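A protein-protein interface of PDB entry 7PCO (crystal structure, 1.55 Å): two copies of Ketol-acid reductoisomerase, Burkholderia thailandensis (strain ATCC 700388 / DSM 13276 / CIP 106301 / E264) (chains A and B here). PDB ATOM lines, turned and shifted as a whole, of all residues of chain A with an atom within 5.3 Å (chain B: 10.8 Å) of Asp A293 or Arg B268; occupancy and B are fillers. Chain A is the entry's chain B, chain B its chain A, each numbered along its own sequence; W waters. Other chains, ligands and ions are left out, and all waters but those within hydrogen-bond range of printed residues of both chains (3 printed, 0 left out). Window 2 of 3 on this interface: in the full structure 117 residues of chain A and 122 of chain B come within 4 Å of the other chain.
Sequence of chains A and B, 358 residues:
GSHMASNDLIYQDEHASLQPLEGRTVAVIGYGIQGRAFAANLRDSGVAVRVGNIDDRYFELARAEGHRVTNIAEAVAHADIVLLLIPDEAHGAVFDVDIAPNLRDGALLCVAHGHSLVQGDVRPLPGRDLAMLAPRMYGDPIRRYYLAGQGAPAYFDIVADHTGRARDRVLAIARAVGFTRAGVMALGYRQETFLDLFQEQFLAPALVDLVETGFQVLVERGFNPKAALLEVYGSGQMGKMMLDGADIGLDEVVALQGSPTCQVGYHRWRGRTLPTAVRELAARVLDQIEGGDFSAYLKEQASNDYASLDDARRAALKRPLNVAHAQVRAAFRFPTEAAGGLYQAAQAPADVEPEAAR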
ATOM      1  N   GLN A 201      11.853  27.495   6.034  1.00  0.00           N
ATOM      2  CA  GLN A 201      11.575  28.355   4.859  1.00  0.00           C
ATOM      3  C   GLN A 201      11.729  29.830   5.219  1.00  0.00           C
ATOM      4  O   GLN A 201      12.085  30.605   4.309  1.00  0.00           O
ATOM      5  CB  GLN A 201      10.179  28.063   4.324  1.00  0.00           C
ATOM      6  CG  GLN A 201      10.114  26.700   3.657  1.00  0.00           C
ATOM      7  CD  GLN A 201       8.712  26.273   3.308  1.00  0.00           C
ATOM      8  OE1 GLN A 201       7.900  27.057   2.816  1.00  0.00           O
ATOM      9  NE2 GLN A 201       8.431  25.003   3.551  1.00  0.00           N
ATOM     10  N   GLN A 288       2.075  30.604   2.393  1.00  0.00           N
ATOM     11  CA  GLN A 288       2.467  29.604   1.364  1.00  0.00           C
ATOM     12  C   GLN A 288       2.395  28.209   1.997  1.00  0.00           C
ATOM     13  O   GLN A 288       1.949  27.258   1.322  1.00  0.00           O
ATOM     14  CB  GLN A 288       3.891  29.847   0.852  1.00  0.00           C
ATOM     15  CG  GLN A 288       4.063  31.047  -0.070  1.00  0.00           C
ATOM     16  CD  GLN A 288       5.504  31.157  -0.515  1.00  0.00           C
ATOM     17  OE1 GLN A 288       6.424  30.816   0.228  1.00  0.00           O
ATOM     18  NE2 GLN A 288       5.714  31.621  -1.736  1.00  0.00           N
ATOM     19  N   GLY A 291      -1.518  27.248   3.118  1.00  0.00           N
ATOM     20  CA  GLY A 291      -2.545  27.283   2.056  1.00  0.00           C
ATOM     21  C   GLY A 291      -2.325  26.232   0.982  1.00  0.00           C
ATOM     22  O   GLY A 291      -3.163  26.163   0.063  1.00  0.00           O
ATOM     23  N   GLY A 292      -1.238  25.455   1.066  1.00  0.00           N
ATOM     24  CA  GLY A 292      -0.961  24.349   0.129  1.00  0.00           C
ATOM     25  C   GLY A 292       0.025  24.719  -0.974  1.00  0.00           C
ATOM     26  O   GLY A 292       0.431  23.799  -1.705  1.00  0.00           O
ATOM     27  N   ASP A 293       0.408  25.997  -1.102  1.00  0.00           N
ATOM     28  CA  ASP A 293       1.338  26.471  -2.168  1.00  0.00           C
ATOM     29  C   ASP A 293       2.664  25.732  -2.020  1.00  0.00           C
ATOM     30  O   ASP A 293       3.199  25.261  -3.038  1.00  0.00           O
ATOM     31  CB  ASP A 293       1.568  27.987  -2.141  1.00  0.00           C
ATOM     32  CG  ASP A 293       2.591  28.487  -3.155  1.00  0.00           C
ATOM     33  OD1 ASP A 293       3.767  28.107  -3.049  1.00  0.00           O
ATOM     34  OD2 ASP A 293       2.201  29.261  -4.046  1.00  0.00           O
ATOM     35  N   PHE A 294       3.208  25.662  -0.803  1.00  0.00           N
ATOM     36  CA  PHE A 294       4.513  24.992  -0.599  1.00  0.00           C
ATOM     37  C   PHE A 294       4.374  23.497  -0.901  1.00  0.00           C
ATOM     38  O   PHE A 294       5.308  22.943  -1.495  1.00  0.00           O
ATOM     39  CB  PHE A 294       5.103  25.202   0.794  1.00  0.00           C
ATOM     40  CG  PHE A 294       6.297  24.314   0.993  1.00  0.00           C
ATOM     41  CD1 PHE A 294       7.490  24.580   0.337  1.00  0.00           C
ATOM     42  CD2 PHE A 294       6.195  23.152   1.743  1.00  0.00           C
ATOM     43  CE1 PHE A 294       8.576  23.733   0.477  1.00  0.00           C
ATOM     44  CE2 PHE A 294       7.281  22.301   1.874  1.00  0.00           C
ATOM     45  CZ  PHE A 294       8.471  22.596   1.243  1.00  0.00           C
ATOM     46  N   SER A 295       3.270  22.857  -0.497  1.00  0.00           N
ATOM     47  CA  SER A 295       3.068  21.401  -0.713  1.00  0.00           C
ATOM     48  C   SER A 295       3.101  21.099  -2.224  1.00  0.00           C
ATOM     49  O   SER A 295       3.713  20.075  -2.623  1.00  0.00           O
ATOM     50  CB  SER A 295       1.797  20.901  -0.030  1.00  0.00           C
ATOM     51  OG  SER A 295       1.873  21.063   1.383  1.00  0.00           O
ATOM     52  N   ALA A 296       2.523  21.976  -3.051  1.00  0.00           N
ATOM     53  CA  ALA A 296       2.470  21.804  -4.522  1.00  0.00           C
ATOM     54  C   ALA A 296       3.878  21.962  -5.114  1.00  0.00           C
ATOM     55  O   ALA A 296       4.249  21.165  -6.002  1.00  0.00           O
ATOM     56  CB  ALA A 296       1.478  22.772  -5.133  1.00  0.00           C
ATOM     57  N   TYR A 297       4.630  22.959  -4.636  1.00  0.00           N
ATOM     58  CA  TYR A 297       6.037  23.261  -5.020  1.00  0.00           C
ATOM     59  C   TYR A 297       6.911  22.044  -4.704  1.00  0.00           C
ATOM     60  O   TYR A 297       7.656  21.577  -5.582  1.00  0.00           O
ATOM     61  CB  TYR A 297       6.533  24.500  -4.270  1.00  0.00           C
ATOM     62  CG  TYR A 297       7.973  24.893  -4.497  1.00  0.00           C
ATOM     63  CD1 TYR A 297       8.338  25.616  -5.623  1.00  0.00           C
ATOM     64  CD2 TYR A 297       8.965  24.594  -3.574  1.00  0.00           C
ATOM     65  CE1 TYR A 297       9.648  26.006  -5.845  1.00  0.00           C
ATOM     66  CE2 TYR A 297      10.282  24.983  -3.777  1.00  0.00           C
ATOM     67  CZ  TYR A 297      10.626  25.693  -4.918  1.00  0.00           C
ATOM     68  OH  TYR A 297      11.909  26.107  -5.144  1.00  0.00           O
ATOM     69  N   LEU A 298       6.816  21.550  -3.469  1.00  0.00           N
ATOM     70  CA  LEU A 298       7.584  20.365  -3.003  1.00  0.00           C
ATOM     71  C   LEU A 298       7.285  19.149  -3.895  1.00  0.00           C
ATOM     72  O   LEU A 298       8.229  18.422  -4.228  1.00  0.00           O
ATOM     73  CB  LEU A 298       7.239  20.081  -1.543  1.00  0.00           C
ATOM     74  CG  LEU A 298       7.793  18.762  -1.013  1.00  0.00           C
ATOM     75  CD1 LEU A 298       9.314  18.792  -0.966  1.00  0.00           C
ATOM     76  CD2 LEU A 298       7.206  18.437   0.349  1.00  0.00           C
ATOM     77  N   ASP B 251      25.334  26.361   4.132  1.00  0.00           N
ATOM     78  CA  ASP B 251      24.548  25.688   3.058  1.00  0.00           C
ATOM     79  C   ASP B 251      24.835  24.180   3.109  1.00  0.00           C
ATOM     80  O   ASP B 251      23.900  23.392   2.895  1.00  0.00           O
ATOM     81  CB  ASP B 251      24.827  26.341   1.701  1.00  0.00           C
ATOM     82  CG  ASP B 251      24.259  27.752   1.631  1.00  0.00           C
ATOM     83  OD1 ASP B 251      23.077  27.927   2.001  1.00  0.00           O
ATOM     84  OD2 ASP B 251      25.009  28.679   1.258  1.00  0.00           O
ATOM     85  N   VAL B 254      22.786  22.206   5.739  1.00  0.00           N
ATOM     86  CA  VAL B 254      21.400  21.924   5.251  1.00  0.00           C
ATOM     87  C   VAL B 254      21.444  20.748   4.266  1.00  0.00           C
ATOM     88  O   VAL B 254      20.591  19.856   4.365  1.00  0.00           O
ATOM     89  CB  VAL B 254      20.747  23.185   4.667  1.00  0.00           C
ATOM     90  CG1 VAL B 254      19.443  22.890   3.947  1.00  0.00           C
ATOM     91  CG2 VAL B 254      20.532  24.215   5.766  1.00  0.00           C
ATOM     92  N   PRO B 260      14.867  16.046   2.603  1.00  0.00           N
ATOM     93  CA  PRO B 260      14.615  16.711   1.331  1.00  0.00           C
ATOM     94  C   PRO B 260      13.546  17.806   1.434  1.00  0.00           C
ATOM     95  O   PRO B 260      13.668  18.783   0.749  1.00  0.00           O
ATOM     96  CB  PRO B 260      14.210  15.550   0.409  1.00  0.00           C
ATOM     97  CG  PRO B 260      14.930  14.353   1.009  1.00  0.00           C
ATOM     98  CD  PRO B 260      14.851  14.576   2.507  1.00  0.00           C
ATOM     99  N   THR B 261      12.522  17.611   2.271  1.00  0.00           N
ATOM    100  CA  THR B 261      11.449  18.604   2.526  1.00  0.00           C
ATOM    101  C   THR B 261      12.098  19.907   3.005  1.00  0.00           C
ATOM    102  O   THR B 261      11.752  20.992   2.480  1.00  0.00           O
ATOM    103  CB  THR B 261      10.456  18.053   3.560  1.00  0.00           C
ATOM    104  OG1 THR B 261       9.965  16.796   3.079  1.00  0.00           O
ATOM    105  CG2 THR B 261       9.319  19.011   3.835  1.00  0.00           C
ATOM    106  N   CYS B 262      13.009  19.787   3.978  1.00  0.00           N
ATOM    107  CA  CYS B 262      13.760  20.914   4.576  1.00  0.00           C
ATOM    108  C   CYS B 262      14.580  21.609   3.482  1.00  0.00           C
ATOM    109  O   CYS B 262      14.469  22.842   3.333  1.00  0.00           O
ATOM    110  CB  CYS B 262      14.653  20.420   5.705  1.00  0.00           C
ATOM    111  SG  CYS B 262      15.766  21.711   6.305  1.00  0.00           S
ATOM    112  N   GLN B 263      15.328  20.843   2.696  1.00  0.00           N
ATOM    113  CA  GLN B 263      16.262  21.406   1.690  1.00  0.00           C
ATOM    114  C   GLN B 263      15.473  22.159   0.614  1.00  0.00           C
ATOM    115  O   GLN B 263      15.880  23.261   0.213  1.00  0.00           O
ATOM    116  CB  GLN B 263      17.118  20.290   1.103  1.00  0.00           C
ATOM    117  CG  GLN B 263      18.036  19.641   2.125  1.00  0.00           C
ATOM    118  CD  GLN B 263      19.120  18.806   1.491  1.00  0.00           C
ATOM    119  OE1 GLN B 263      19.697  19.183   0.477  1.00  0.00           O
ATOM    120  NE2 GLN B 263      19.417  17.670   2.100  1.00  0.00           N
ATOM    121  N   VAL B 264      14.373  21.578   0.146  1.00  0.00           N
ATOM    122  CA  VAL B 264      13.521  22.229  -0.885  1.00  0.00           C
ATOM    123  C   VAL B 264      12.982  23.547  -0.312  1.00  0.00           C
ATOM    124  O   VAL B 264      12.996  24.556  -1.032  1.00  0.00           O
ATOM    125  CB  VAL B 264      12.391  21.288  -1.336  1.00  0.00           C
ATOM    126  CG1 VAL B 264      11.344  22.043  -2.135  1.00  0.00           C
ATOM    127  CG2 VAL B 264      12.933  20.112  -2.129  1.00  0.00           C
ATOM    128  N   GLY B 265      12.476  23.536   0.927  1.00  0.00           N
ATOM    129  CA  GLY B 265      11.947  24.757   1.560  1.00  0.00           C
ATOM    130  C   GLY B 265      13.028  25.820   1.717  1.00  0.00           C
ATOM    131  O   GLY B 265      12.795  26.994   1.341  1.00  0.00           O
ATOM    132  N   TYR B 266      14.177  25.424   2.250  1.00  0.00           N
ATOM    133  CA  TYR B 266      15.331  26.321   2.525  1.00  0.00           C
ATOM    134  C   TYR B 266      15.761  27.024   1.233  1.00  0.00           C
ATOM    135  O   TYR B 266      15.917  28.254   1.245  1.00  0.00           O
ATOM    136  CB  TYR B 266      16.464  25.515   3.159  1.00  0.00           C
ATOM    137  CG  TYR B 266      17.761  26.250   3.376  1.00  0.00           C
ATOM    138  CD1 TYR B 266      18.802  26.147   2.466  1.00  0.00           C
ATOM    139  CD2 TYR B 266      17.976  26.998   4.525  1.00  0.00           C
ATOM    140  CE1 TYR B 266      20.014  26.790   2.679  1.00  0.00           C
ATOM    141  CE2 TYR B 266      19.178  27.649   4.753  1.00  0.00           C
ATOM    142  CZ  TYR B 266      20.204  27.540   3.829  1.00  0.00           C
ATOM    143  OH  TYR B 266      21.395  28.163   4.059  1.00  0.00           O
ATOM    144  N   HIS B 267      15.891  26.275   0.137  1.00  0.00           N
ATOM    145  CA  HIS B 267      16.407  26.814  -1.150  1.00  0.00           C
ATOM    146  C   HIS B 267      15.321  27.614  -1.881  1.00  0.00           C
ATOM    147  O   HIS B 267      15.681  28.345  -2.817  1.00  0.00           O
ATOM    148  CB  HIS B 267      17.028  25.698  -2.000  1.00  0.00           C
ATOM    149  CG  HIS B 267      18.403  25.346  -1.551  1.00  0.00           C
ATOM    150  ND1 HIS B 267      19.458  26.234  -1.655  1.00  0.00           N
ATOM    151  CD2 HIS B 267      18.892  24.239  -0.955  1.00  0.00           C
ATOM    152  CE1 HIS B 267      20.544  25.678  -1.154  1.00  0.00           C
ATOM    153  NE2 HIS B 267      20.220  24.450  -0.718  1.00  0.00           N
ATOM    154  N   ARG B 268      14.046  27.507  -1.488  1.00  0.00           N
ATOM    155  CA  ARG B 268      12.978  28.373  -2.062  1.00  0.00           C
ATOM    156  C   ARG B 268      13.263  29.833  -1.681  1.00  0.00           C
ATOM    157  O   ARG B 268      12.983  30.733  -2.497  1.00  0.00           O
ATOM    158  CB  ARG B 268      11.577  27.982  -1.578  1.00  0.00           C
ATOM    159  CG  ARG B 268      10.470  28.586  -2.432  1.00  0.00           C
ATOM    160  CD  ARG B 268       9.082  28.094  -2.082  1.00  0.00           C
ATOM    161  NE  ARG B 268       8.157  28.423  -3.156  1.00  0.00           N
ATOM    162  CZ  ARG B 268       6.841  28.319  -3.076  1.00  0.00           C
ATOM    163  NH1 ARG B 268       6.285  27.922  -1.946  1.00  0.00           N
ATOM    164  NH2 ARG B 268       6.087  28.643  -4.114  1.00  0.00           N
ATOM    165  N   TRP B 269      13.787  30.068  -0.478  1.00  0.00           N
ATOM    166  CA  TRP B 269      13.896  31.434   0.098  1.00  0.00           C
ATOM    167  C   TRP B 269      15.349  31.844   0.359  1.00  0.00           C
ATOM    168  O   TRP B 269      15.572  33.044   0.534  1.00  0.00           O
ATOM    169  CB  TRP B 269      13.010  31.538   1.344  1.00  0.00           C
ATOM    170  CG  TRP B 269      11.571  31.712   0.966  1.00  0.00           C
ATOM    171  CD1 TRP B 269      10.585  30.770   0.992  1.00  0.00           C
ATOM    172  CD2 TRP B 269      10.972  32.905   0.427  1.00  0.00           C
ATOM    173  NE1 TRP B 269       9.409  31.307   0.541  1.00  0.00           N
ATOM    174  CE2 TRP B 269       9.618  32.609   0.175  1.00  0.00           C
ATOM    175  CE3 TRP B 269      11.449  34.190   0.136  1.00  0.00           C
ATOM    176  CZ2 TRP B 269       8.733  33.556  -0.342  1.00  0.00           C
ATOM    177  CZ3 TRP B 269      10.575  35.125  -0.374  1.00  0.00           C
ATOM    178  CH2 TRP B 269       9.237  34.809  -0.614  1.00  0.00           C
ATOM    179  N   ARG B 270      16.302  30.908   0.370  1.00  0.00           N
ATOM    180  CA  ARG B 270      17.748  31.224   0.496  1.00  0.00           C
ATOM    181  C   ARG B 270      18.116  32.315  -0.517  1.00  0.00           C
ATOM    182  O   ARG B 270      17.792  32.171  -1.711  1.00  0.00           O
ATOM    183  CB  ARG B 270      18.583  29.952   0.311  1.00  0.00           C
ATOM    184  CG  ARG B 270      20.083  30.156   0.455  1.00  0.00           C
ATOM    185  CD  ARG B 270      20.531  30.630   1.826  1.00  0.00           C
ATOM    186  NE  ARG B 270      21.982  30.635   1.738  1.00  0.00           N
ATOM    187  CZ  ARG B 270      22.755  31.693   1.487  1.00  0.00           C
ATOM    188  NH1 ARG B 270      22.255  32.916   1.396  1.00  0.00           N
ATOM    189  NH2 ARG B 270      24.058  31.517   1.370  1.00  0.00           N
ATOM    190  N   GLY B 271      18.737  33.392  -0.040  1.00  0.00           N
ATOM    191  CA  GLY B 271      19.184  34.519  -0.880  1.00  0.00           C
ATOM    192  C   GLY B 271      18.061  35.491  -1.192  1.00  0.00           C
ATOM    193  O   GLY B 271      18.320  36.430  -1.950  1.00  0.00           O
ATOM    194  N   ARG B 272      16.858  35.304  -0.630  1.00  0.00           N
ATOM    195  CA  ARG B 272      15.667  36.102  -1.036  1.00  0.00           C
ATOM    196  C   ARG B 272      14.917  36.715   0.159  1.00  0.00           C
ATOM    197  O   ARG B 272      13.913  37.379  -0.111  1.00  0.00           O
ATOM    198  CB  ARG B 272      14.708  35.235  -1.861  1.00  0.00           C
ATOM    199  CG  ARG B 272      15.362  34.497  -3.022  1.00  0.00           C
ATOM    200  CD  ARG B 272      14.380  33.685  -3.856  1.00  0.00           C
ATOM    201  NE  ARG B 272      13.154  34.423  -4.166  1.00  0.00           N
ATOM    202  CZ  ARG B 272      11.903  34.070  -3.837  1.00  0.00           C
ATOM    203  NH1 ARG B 272      10.895  34.851  -4.187  1.00  0.00           N
ATOM    204  NH2 ARG B 272      11.646  32.951  -3.176  1.00  0.00           N
ATOM    205  N   THR B 273      15.354  36.536   1.416  1.00  0.00           N
ATOM    206  CA  THR B 273      14.509  36.866   2.602  1.00  0.00           C
ATOM    207  C   THR B 273      14.626  38.340   3.003  1.00  0.00           C
ATOM    208  O   THR B 273      13.694  38.815   3.654  1.00  0.00           O
ATOM    209  CB  THR B 273      14.808  35.995   3.830  1.00  0.00           C
ATOM    210  OG1 THR B 273      16.175  36.189   4.194  1.00  0.00           O
ATOM    211  CG2 THR B 273      14.511  34.528   3.605  1.00  0.00           C
ATOM    212  N   LEU B 274      15.713  39.040   2.658  1.00  0.00           N
ATOM    213  CA  LEU B 274      16.005  40.380   3.245  1.00  0.00           C
ATOM    214  C   LEU B 274      15.818  41.502   2.227  1.00  0.00           C
ATOM    215  O   LEU B 274      16.318  41.426   1.110  1.00  0.00           O
ATOM    216  CB  LEU B 274      17.429  40.382   3.803  1.00  0.00           C
ATOM    217  CG  LEU B 274      17.753  39.245   4.770  1.00  0.00           C
ATOM    218  CD1 LEU B 274      19.187  39.356   5.254  1.00  0.00           C
ATOM    219  CD2 LEU B 274      16.797  39.226   5.954  1.00  0.00           C
HETATM  220  O   HOH W   1      13.775  25.043  -3.569  1.00  0.00           O
HETATM  221  O   HOH W   2       7.160  28.359   0.824  1.00  0.00           O
HETATM  222  O   HOH W   3      10.790  23.098   4.230  1.00  0.00           O
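Among the printed residues, pairs that only touch across the chains: Gln A201 with Gly B265, Gln A201 with Trp B269, Gln A288 with Arg B268, Phe A294 with Thr B261, Phe A294 with Gly B265, Phe A294 with Arg B268, Tyr A297 with Val B264, Tyr A297 with Arg B268 and Leu A298 with Val B264.
Of chain B, only Arg B268 and Trp B269 come within 4 Å of Gln A288. No residue of chain B comes within 4 Å of Gly A291. Printed residues of chain B within 4 Å of Asp A293: Arg B268. Of the printed residues of chain B, Phe A294 touches Thr B261 (3.9 Å), Gly B265 (3.7 Å) and Arg B268 (3.7 Å). No residue of chain B comes within 4 Å of Ser A295. Of the printed residues of chain B, Leu A298 touches Val B264. Cys B262 touches none of the printed residues of chain A. Of the printed residues of chain A, Val B264 touches Tyr A297 (3.5 Å) and Leu A298 (3.98 Å). Of the printed residues of chain A, Gly B265 touches Gln A201 and Phe A294. Arg B268 touches just these residues of chain A: Gln A288, Asp A293, Phe A294 and Tyr A297. Of the printed residues of chain A, Trp B269 touches Gln A201 and Gln A288. The nearest residue of chain A that does not touch Arg B268 is Gln A201 (5.1 Å).
No position is printed for both chains. Of the 11 pairs that touch across the chains among the printed residues, none has its exchanged pair printed and touching as well.
The backbone carbonyl oxygen (O) of Arg B268 sits at hydrogen-bond distance from the guanidinium group (NH2) of Arg B272, 2.7 Å away. N of Asp A293 lies within hydrogen-bond range of O of Gln A288 (3.1 Å). The backbone carbonyl oxygen of Gln A288 is in hydrogen-bond range of the backbone NH of Phe A294, 2.9 Å away.
Water W2 lies within hydrogen-bond range of OE1 of Gln A201, OE1 of Gln A288 and NH1 of Arg B268. Water W1 lies within hydrogen-bond range of the side-chain hydroxyl (OH) of Tyr A297, the backbone carbonyl oxygen (O) of Val B264 and the backbone NH (N) of Arg B268. Water W3 lies within hydrogen-bond range of O of Thr B261 (2.9 Å) and NE2 of Gln A201 (3.1 Å).
The side-chain carboxylate of Asp A293 is in salt-bridge range of the guanidinium group of Arg B268, 2.6 Å away. The indole nitrogen of Trp B269 is in hydrogen-bond range of the side-chain amide oxygen of Gln A288 (3.0 Å).
Printed residues of chain A that touch a printed residue of chain B: Gln A201, Gln A288, Asp A293, Phe A294, Tyr A297 and Leu A298. Hydrophobic or aromatic side chains of chain A within 4 Å of the printed part of chain B: Phe A294, Tyr A297 and Leu A298. Printed residues of chain B that touch a printed residue of chain A: Thr B261, Val B264, Gly B265, Arg B268 and Trp B269. Hydrophobic or aromatic side chains of chain B within 4 Å of the printed part of chain A: Val B264 and Trp B269. Among the printed residues, Asp or Glu carboxylates within 4 Å of a Lys or Arg side-chain nitrogen of the other chain: Asp A293 with Arg B268.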
